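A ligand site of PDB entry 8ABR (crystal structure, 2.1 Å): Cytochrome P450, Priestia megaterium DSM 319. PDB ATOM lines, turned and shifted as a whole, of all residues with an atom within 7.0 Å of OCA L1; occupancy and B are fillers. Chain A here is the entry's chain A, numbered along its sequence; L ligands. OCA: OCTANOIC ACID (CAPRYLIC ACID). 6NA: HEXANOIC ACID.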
ATOM      1  N   GLU A  78     -23.674  -0.272   4.330  1.00  0.00           N
ATOM      2  CA  GLU A  78     -22.904  -1.515   4.334  1.00  0.00           C
ATOM      3  C   GLU A  78     -23.290  -2.404   3.160  1.00  0.00           C
ATOM      4  O   GLU A  78     -24.302  -2.209   2.486  1.00  0.00           O
ATOM      5  CB  GLU A  78     -23.086  -2.256   5.668  1.00  0.00           C
ATOM      6  CG  GLU A  78     -22.018  -3.316   5.949  1.00  0.00           C
ATOM      7  CD  GLU A  78     -21.687  -3.422   7.425  1.00  0.00           C
ATOM      8  OE1 GLU A  78     -22.425  -2.856   8.256  1.00  0.00           O
ATOM      9  OE2 GLU A  78     -20.675  -4.075   7.754  1.00  0.00           O
ATOM     10  N   ARG A  79     -22.438  -3.389   2.910  1.00  0.00           N
ATOM     11  CA  ARG A  79     -22.510  -4.231   1.709  1.00  0.00           C
ATOM     12  C   ARG A  79     -23.429  -5.428   1.954  1.00  0.00           C
ATOM     13  O   ARG A  79     -23.006  -6.576   2.109  1.00  0.00           O
ATOM     14  CB  ARG A  79     -21.101  -4.648   1.308  1.00  0.00           C
ATOM     15  CG  ARG A  79     -20.070  -4.731   2.449  1.00  0.00           C
ATOM     16  CD  ARG A  79     -19.440  -3.372   2.815  1.00  0.00           C
ATOM     17  NE  ARG A  79     -19.060  -3.265   4.219  1.00  0.00           N
ATOM     18  CZ  ARG A  79     -17.818  -3.060   4.669  1.00  0.00           C
ATOM     19  NH1 ARG A  79     -16.802  -2.893   3.839  1.00  0.00           N
ATOM     20  NH2 ARG A  79     -17.595  -3.024   5.980  1.00  0.00           N
ATOM     21  N   GLN A  80     -24.740  -5.128   1.981  1.00  0.00           N
ATOM     22  CA  GLN A  80     -25.766  -6.116   2.322  1.00  0.00           C
ATOM     23  C   GLN A  80     -26.961  -5.971   1.384  1.00  0.00           C
ATOM     24  O   GLN A  80     -28.039  -5.486   1.741  1.00  0.00           O
ATOM     25  CB  GLN A  80     -26.179  -5.977   3.796  1.00  0.00           C
ATOM     26  CG  GLN A  80     -25.024  -6.143   4.773  1.00  0.00           C
ATOM     27  CD  GLN A  80     -25.410  -5.984   6.230  1.00  0.00           C
ATOM     28  OE1 GLN A  80     -26.475  -6.408   6.656  1.00  0.00           O
ATOM     29  NE2 GLN A  80     -24.539  -5.365   7.010  1.00  0.00           N
ATOM     30  N   SER A  82     -29.057  -8.109   0.352  1.00  0.00           N
ATOM     31  CA  SER A  82     -29.753  -9.363   0.611  1.00  0.00           C
ATOM     32  C   SER A  82     -31.193  -9.066   1.017  1.00  0.00           C
ATOM     33  O   SER A  82     -31.545  -7.951   1.401  1.00  0.00           O
ATOM     34  CB  SER A  82     -29.068 -10.167   1.727  1.00  0.00           C
ATOM     35  OG  SER A  82     -29.472  -9.642   2.984  1.00  0.00           O
ATOM     36  N   LEU A  84     -32.726  -9.765   3.580  1.00  0.00           N
ATOM     37  CA  LEU A  84     -32.841  -9.295   4.955  1.00  0.00           C
ATOM     38  C   LEU A  84     -33.043  -7.788   5.015  1.00  0.00           C
ATOM     39  O   LEU A  84     -33.799  -7.291   5.855  1.00  0.00           O
ATOM     40  CB  LEU A  84     -31.593  -9.668   5.751  1.00  0.00           C
ATOM     41  CG  LEU A  84     -31.550  -9.205   7.210  1.00  0.00           C
ATOM     42  CD1 LEU A  84     -32.634  -9.893   8.005  1.00  0.00           C
ATOM     43  CD2 LEU A  84     -30.168  -9.459   7.845  1.00  0.00           C
ATOM     44  N   MET A  85     -32.403  -7.050   4.094  1.00  0.00           N
ATOM     45  CA  MET A  85     -32.397  -5.593   4.104  1.00  0.00           C
ATOM     46  C   MET A  85     -33.295  -5.008   3.033  1.00  0.00           C
ATOM     47  O   MET A  85     -33.148  -3.822   2.695  1.00  0.00           O
ATOM     48  CB  MET A  85     -30.972  -5.071   3.938  1.00  0.00           C
ATOM     49  CG  MET A  85     -29.974  -5.609   4.931  1.00  0.00           C
ATOM     50  SD  MET A  85     -29.962  -4.675   6.460  1.00  0.00           S
ATOM     51  CE  MET A  85     -29.109  -5.799   7.564  1.00  0.00           C
ATOM     52  N   SER A 164     -17.179 -15.396   9.430  1.00  0.00           N
ATOM     53  CA  SER A 164     -18.618 -15.315   9.617  1.00  0.00           C
ATOM     54  C   SER A 164     -18.949 -14.608  10.934  1.00  0.00           C
ATOM     55  O   SER A 164     -19.801 -13.715  10.982  1.00  0.00           O
ATOM     56  CB  SER A 164     -19.230 -16.723   9.577  1.00  0.00           C
ATOM     57  OG  SER A 164     -20.603 -16.643   9.858  1.00  0.00           O
ATOM     58  N   ASP A 166     -17.168 -12.460  12.404  1.00  0.00           N
ATOM     59  CA  ASP A 166     -16.821 -11.052  12.237  1.00  0.00           C
ATOM     60  C   ASP A 166     -18.019 -10.226  11.776  1.00  0.00           C
ATOM     61  O   ASP A 166     -18.170  -9.081  12.192  1.00  0.00           O
ATOM     62  CB  ASP A 166     -15.699 -10.886  11.209  1.00  0.00           C
ATOM     63  CG  ASP A 166     -14.302 -11.092  11.799  1.00  0.00           C
ATOM     64  OD1 ASP A 166     -14.112 -11.210  13.031  1.00  0.00           O
ATOM     65  OD2 ASP A 166     -13.365 -11.114  10.985  1.00  0.00           O
ATOM     66  N   LEU A 167     -18.860 -10.793  10.908  1.00  0.00           N
ATOM     67  CA  LEU A 167     -19.926 -10.019  10.284  1.00  0.00           C
ATOM     68  C   LEU A 167     -21.109  -9.799  11.210  1.00  0.00           C
ATOM     69  O   LEU A 167     -22.076  -9.148  10.808  1.00  0.00           O
ATOM     70  CB  LEU A 167     -20.417 -10.736   9.009  1.00  0.00           C
ATOM     71  CG  LEU A 167     -19.459 -10.849   7.834  1.00  0.00           C
ATOM     72  CD1 LEU A 167     -20.176 -11.425   6.613  1.00  0.00           C
ATOM     73  CD2 LEU A 167     -18.830  -9.516   7.490  1.00  0.00           C
ATOM     74  N   VAL A 168     -21.059 -10.349  12.423  1.00  0.00           N
ATOM     75  CA  VAL A 168     -22.099 -10.195  13.440  1.00  0.00           C
ATOM     76  C   VAL A 168     -21.605  -9.403  14.641  1.00  0.00           C
ATOM     77  O   VAL A 168     -22.414  -9.027  15.497  1.00  0.00           O
ATOM     78  CB  VAL A 168     -22.624 -11.584  13.873  1.00  0.00           C
ATOM     79  CG1 VAL A 168     -23.090 -11.589  15.286  1.00  0.00           C
ATOM     80  CG2 VAL A 168     -23.739 -12.066  12.930  1.00  0.00           C
ATOM     81  N   ARG A 186     -15.410  -6.134  11.105  1.00  0.00           N
ATOM     82  CA  ARG A 186     -16.416  -6.491  10.103  1.00  0.00           C
ATOM     83  C   ARG A 186     -15.824  -6.433   8.695  1.00  0.00           C
ATOM     84  O   ARG A 186     -16.137  -7.279   7.841  1.00  0.00           O
ATOM     85  CB  ARG A 186     -17.639  -5.573  10.220  1.00  0.00           C
ATOM     86  CG  ARG A 186     -18.504  -5.852  11.466  1.00  0.00           C
ATOM     87  CD  ARG A 186     -19.524  -4.742  11.765  1.00  0.00           C
ATOM     88  NE  ARG A 186     -20.669  -4.765  10.854  1.00  0.00           N
ATOM     89  CZ  ARG A 186     -21.757  -5.494  11.067  1.00  0.00           C
ATOM     90  NH1 ARG A 186     -21.894  -6.248  12.144  1.00  0.00           N
ATOM     91  NH2 ARG A 186     -22.741  -5.449  10.166  1.00  0.00           N
ATOM     92  N   VAL A 190     -15.788  -9.203   5.484  1.00  0.00           N
ATOM     93  CA  VAL A 190     -16.305  -8.849   4.166  1.00  0.00           C
ATOM     94  C   VAL A 190     -15.257  -9.149   3.098  1.00  0.00           C
ATOM     95  O   VAL A 190     -15.558  -9.752   2.058  1.00  0.00           O
ATOM     96  CB  VAL A 190     -16.723  -7.363   4.140  1.00  0.00           C
ATOM     97  CG1 VAL A 190     -17.123  -6.940   2.727  1.00  0.00           C
ATOM     98  CG2 VAL A 190     -17.847  -7.102   5.115  1.00  0.00           C
ATOM     99  N   GLN A 194     -16.610 -12.027   0.797  1.00  0.00           N
ATOM    100  CA  GLN A 194     -17.023 -11.548  -0.518  1.00  0.00           C
ATOM    101  C   GLN A 194     -16.104 -12.113  -1.580  1.00  0.00           C
ATOM    102  O   GLN A 194     -16.547 -12.545  -2.647  1.00  0.00           O
ATOM    103  CB  GLN A 194     -16.982 -10.016  -0.582  1.00  0.00           C
ATOM    104  CG  GLN A 194     -18.186  -9.327  -0.055  1.00  0.00           C
ATOM    105  CD  GLN A 194     -18.385  -7.953  -0.696  1.00  0.00           C
ATOM    106  OE1 GLN A 194     -17.520  -7.456  -1.423  1.00  0.00           O
ATOM    107  NE2 GLN A 194     -19.553  -7.361  -0.463  1.00  0.00           N
ATOM    108  N   GLY A 233     -25.222 -11.349  -2.077  1.00  0.00           N
ATOM    109  CA  GLY A 233     -25.986 -11.075  -0.869  1.00  0.00           C
ATOM    110  C   GLY A 233     -26.666 -12.318  -0.341  1.00  0.00           C
ATOM    111  O   GLY A 233     -26.639 -12.594   0.865  1.00  0.00           O
ATOM    112  N   ILE A 236     -23.777 -14.740   1.271  1.00  0.00           N
ATOM    113  CA  ILE A 236     -23.254 -14.375   2.587  1.00  0.00           C
ATOM    114  C   ILE A 236     -24.349 -14.465   3.645  1.00  0.00           C
ATOM    115  O   ILE A 236     -24.131 -14.998   4.737  1.00  0.00           O
ATOM    116  CB  ILE A 236     -22.599 -12.981   2.548  1.00  0.00           C
ATOM    117  CG1 ILE A 236     -21.317 -13.075   1.699  1.00  0.00           C
ATOM    118  CG2 ILE A 236     -22.294 -12.482   3.930  1.00  0.00           C
ATOM    119  CD1 ILE A 236     -20.832 -11.761   1.121  1.00  0.00           C
ATOM    120  N   LEU A 237     -25.527 -13.934   3.333  1.00  0.00           N
ATOM    121  CA  LEU A 237     -26.609 -13.991   4.328  1.00  0.00           C
ATOM    122  C   LEU A 237     -26.895 -15.431   4.701  1.00  0.00           C
ATOM    123  O   LEU A 237     -26.920 -15.796   5.882  1.00  0.00           O
ATOM    124  CB  LEU A 237     -27.870 -13.310   3.796  1.00  0.00           C
ATOM    125  CG  LEU A 237     -29.168 -13.499   4.582  1.00  0.00           C
ATOM    126  CD1 LEU A 237     -29.042 -12.961   6.007  1.00  0.00           C
ATOM    127  CD2 LEU A 237     -30.323 -12.822   3.841  1.00  0.00           C
ATOM    128  N   LEU A 238     -27.049 -16.300   3.697  1.00  0.00           N
ATOM    129  CA  LEU A 238     -27.349 -17.696   3.984  1.00  0.00           C
ATOM    130  C   LEU A 238     -26.223 -18.355   4.762  1.00  0.00           C
ATOM    131  O   LEU A 238     -26.485 -19.158   5.667  1.00  0.00           O
ATOM    132  CB  LEU A 238     -27.598 -18.447   2.675  1.00  0.00           C
ATOM    133  CG  LEU A 238     -28.957 -18.228   2.018  1.00  0.00           C
ATOM    134  CD1 LEU A 238     -29.011 -18.881   0.636  1.00  0.00           C
ATOM    135  CD2 LEU A 238     -30.084 -18.733   2.916  1.00  0.00           C
ATOM    136  N   VAL A 240     -23.925 -16.855   6.885  1.00  0.00           N
ATOM    137  CA  VAL A 240     -23.809 -16.334   8.243  1.00  0.00           C
ATOM    138  C   VAL A 240     -25.025 -16.718   9.065  1.00  0.00           C
ATOM    139  O   VAL A 240     -24.882 -17.209  10.198  1.00  0.00           O
ATOM    140  CB  VAL A 240     -23.638 -14.803   8.219  1.00  0.00           C
ATOM    141  CG1 VAL A 240     -23.655 -14.261   9.634  1.00  0.00           C
ATOM    142  CG2 VAL A 240     -22.363 -14.405   7.497  1.00  0.00           C
ATOM    143  N   ALA A 241     -26.230 -16.424   8.551  1.00  0.00           N
ATOM    144  CA  ALA A 241     -27.446 -16.797   9.266  1.00  0.00           C
ATOM    145  C   ALA A 241     -27.500 -18.298   9.498  1.00  0.00           C
ATOM    146  O   ALA A 241     -27.874 -18.761  10.576  1.00  0.00           O
ATOM    147  CB  ALA A 241     -28.691 -16.315   8.510  1.00  0.00           C
ATOM    148  N   GLY A 242     -27.137 -19.082   8.495  1.00  0.00           N
ATOM    149  CA  GLY A 242     -27.222 -20.522   8.648  1.00  0.00           C
ATOM    150  C   GLY A 242     -26.368 -21.150   9.752  1.00  0.00           C
ATOM    151  O   GLY A 242     -26.720 -22.202  10.283  1.00  0.00           O
ATOM    152  N   GLU A 244     -24.230 -19.082  12.409  1.00  0.00           N
ATOM    153  CA  GLU A 244     -23.885 -18.378  13.648  1.00  0.00           C
ATOM    154  C   GLU A 244     -25.018 -18.512  14.667  1.00  0.00           C
ATOM    155  O   GLU A 244     -24.801 -18.691  15.864  1.00  0.00           O
ATOM    156  CB  GLU A 244     -23.596 -16.901  13.368  1.00  0.00           C
ATOM    157  CG  GLU A 244     -22.889 -16.143  14.505  1.00  0.00           C
ATOM    158  CD  GLU A 244     -23.835 -15.635  15.605  1.00  0.00           C
ATOM    159  OE1 GLU A 244     -25.053 -15.602  15.397  1.00  0.00           O
ATOM    160  OE2 GLU A 244     -23.337 -15.267  16.690  1.00  0.00           O
ATOM    161  N   THR A 245     -26.247 -18.425  14.193  1.00  0.00           N
ATOM    162  CA  THR A 245     -27.397 -18.574  15.071  1.00  0.00           C
ATOM    163  C   THR A 245     -27.563 -20.008  15.535  1.00  0.00           C
ATOM    164  O   THR A 245     -27.790 -20.272  16.730  1.00  0.00           O
ATOM    165  CB  THR A 245     -28.634 -18.107  14.309  1.00  0.00           C
ATOM    166  OG1 THR A 245     -28.691 -18.853  13.080  1.00  0.00           O
ATOM    167  CG2 THR A 245     -28.591 -16.628  13.989  1.00  0.00           C
ATOM    168  N   ILE A 288     -30.796 -14.712  18.616  1.00  0.00           N
ATOM    169  CA  ILE A 288     -30.943 -13.325  18.179  1.00  0.00           C
ATOM    170  C   ILE A 288     -31.814 -12.621  19.210  1.00  0.00           C
ATOM    171  O   ILE A 288     -32.956 -13.025  19.453  1.00  0.00           O
ATOM    172  CB  ILE A 288     -31.551 -13.228  16.780  1.00  0.00           C
ATOM    173  CG1 ILE A 288     -30.640 -13.866  15.719  1.00  0.00           C
ATOM    174  CG2 ILE A 288     -31.833 -11.776  16.440  1.00  0.00           C
ATOM    175  CD1 ILE A 288     -29.318 -13.186  15.518  1.00  0.00           C
ATOM    176  N   PHE A 389     -26.871  -7.698  19.889  1.00  0.00           N
ATOM    177  CA  PHE A 389     -28.063  -8.342  19.348  1.00  0.00           C
ATOM    178  C   PHE A 389     -27.947  -9.859  19.282  1.00  0.00           C
ATOM    179  O   PHE A 389     -28.896 -10.536  18.853  1.00  0.00           O
ATOM    180  CB  PHE A 389     -28.412  -7.750  17.969  1.00  0.00           C
ATOM    181  CG  PHE A 389     -27.596  -8.294  16.808  1.00  0.00           C
ATOM    182  CD1 PHE A 389     -28.018  -9.410  16.108  1.00  0.00           C
ATOM    183  CD2 PHE A 389     -26.452  -7.641  16.387  1.00  0.00           C
ATOM    184  CE1 PHE A 389     -27.327  -9.895  15.035  1.00  0.00           C
ATOM    185  CE2 PHE A 389     -25.734  -8.145  15.310  1.00  0.00           C
ATOM    186  CZ  PHE A 389     -26.200  -9.270  14.612  1.00  0.00           C
ATOM    187  N   VAL A 390     -26.838 -10.424  19.740  1.00  0.00           N
ATOM    188  CA  VAL A 390     -26.606 -11.862  19.795  1.00  0.00           C
ATOM    189  C   VAL A 390     -26.550 -12.289  21.244  1.00  0.00           C
ATOM    190  O   VAL A 390     -26.095 -11.531  22.112  1.00  0.00           O
ATOM    191  CB  VAL A 390     -25.271 -12.240  19.092  1.00  0.00           C
ATOM    192  CG1 VAL A 390     -24.879 -13.671  19.425  1.00  0.00           C
ATOM    193  CG2 VAL A 390     -25.371 -12.046  17.577  1.00  0.00           C
HETATM  194  C1  OCA L   1     -22.860  -8.039   6.550  1.00  0.00           C
HETATM  195  C2  OCA L   1     -23.657  -9.341   6.262  1.00  0.00           C
HETATM  196  C3  OCA L   1     -25.113  -9.379   6.724  1.00  0.00           C
HETATM  197  C4  OCA L   1     -25.629 -10.798   6.916  1.00  0.00           C
HETATM  198  C5  OCA L   1     -25.722 -11.237   8.369  1.00  0.00           C
HETATM  199  C6  OCA L   1     -26.996 -10.814   9.100  1.00  0.00           C
HETATM  200  C7  OCA L   1     -27.044 -11.196  10.568  1.00  0.00           C
HETATM  201  C8  OCA L   1     -26.949 -12.674  10.834  1.00  0.00           C
HETATM  202  O1  OCA L   1     -22.350  -7.413   5.601  1.00  0.00           O
HETATM  203  O2  OCA L   1     -22.801  -7.699   7.753  1.00  0.00           O
HETATM  204  CA  6NA L   2     -30.440  -8.923  12.974  1.00  0.00           C
HETATM  205  C   6NA L   2     -30.753  -7.425  12.975  1.00  0.00           C
HETATM  206  O   6NA L   2     -29.814  -6.639  13.038  1.00  0.00           O
HETATM  207  CB  6NA L   2     -31.598  -9.888  12.726  1.00  0.00           C
HETATM  208  CG  6NA L   2     -31.102 -11.320  12.569  1.00  0.00           C
HETATM  209  CD  6NA L   2     -31.104 -11.820  11.131  1.00  0.00           C
HETATM  210  C6  6NA L   2     -30.499 -13.219  11.005  1.00  0.00           C
HETATM  211  OXT 6NA L   2     -31.969  -7.105  12.902  1.00  0.00           O
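The guanidinium group (NH2) of Arg 186 lies within salt-bridge range of an oxygen (O2) of OCA L1 (3.3 Å). NE2 of Gln 80 is in hydrogen-bond range of O2 of OCA L1 (3.0 Å).
O of Leu 167 lies within hydrogen-bond range of NH1 of Arg 186 (3.2 Å). The guanidinium group of Arg 79 is in salt-bridge range of the side-chain carboxylate of Glu 78 (3.7 Å). The side-chain carboxylate (OE2) of Glu 78 lies within salt-bridge range of the guanidinium group (NE) of Arg 186, at 3.2 Å. The side-chain hydroxyl (OG) of Ser 82 lies close to the backbone NH (N) of Leu 84.
O2 of OCA L1 sits close to O of Leu 167, 3.5 Å away. Merely in contact with OCA L1: Arg 79 (3.7 Å), Leu 84 (3.7 Å), Val 240 (3.8 Å) and Val 168 (3.9 Å). Of the 25 residues printed, 7 come within 4 Å of OCA L1. Along chain A the residues within 4 Å of OCA L1 span positions 79 to 240. The nearest printed residue that does not touch OCA L1 is Glu 78 (4.1 Å).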
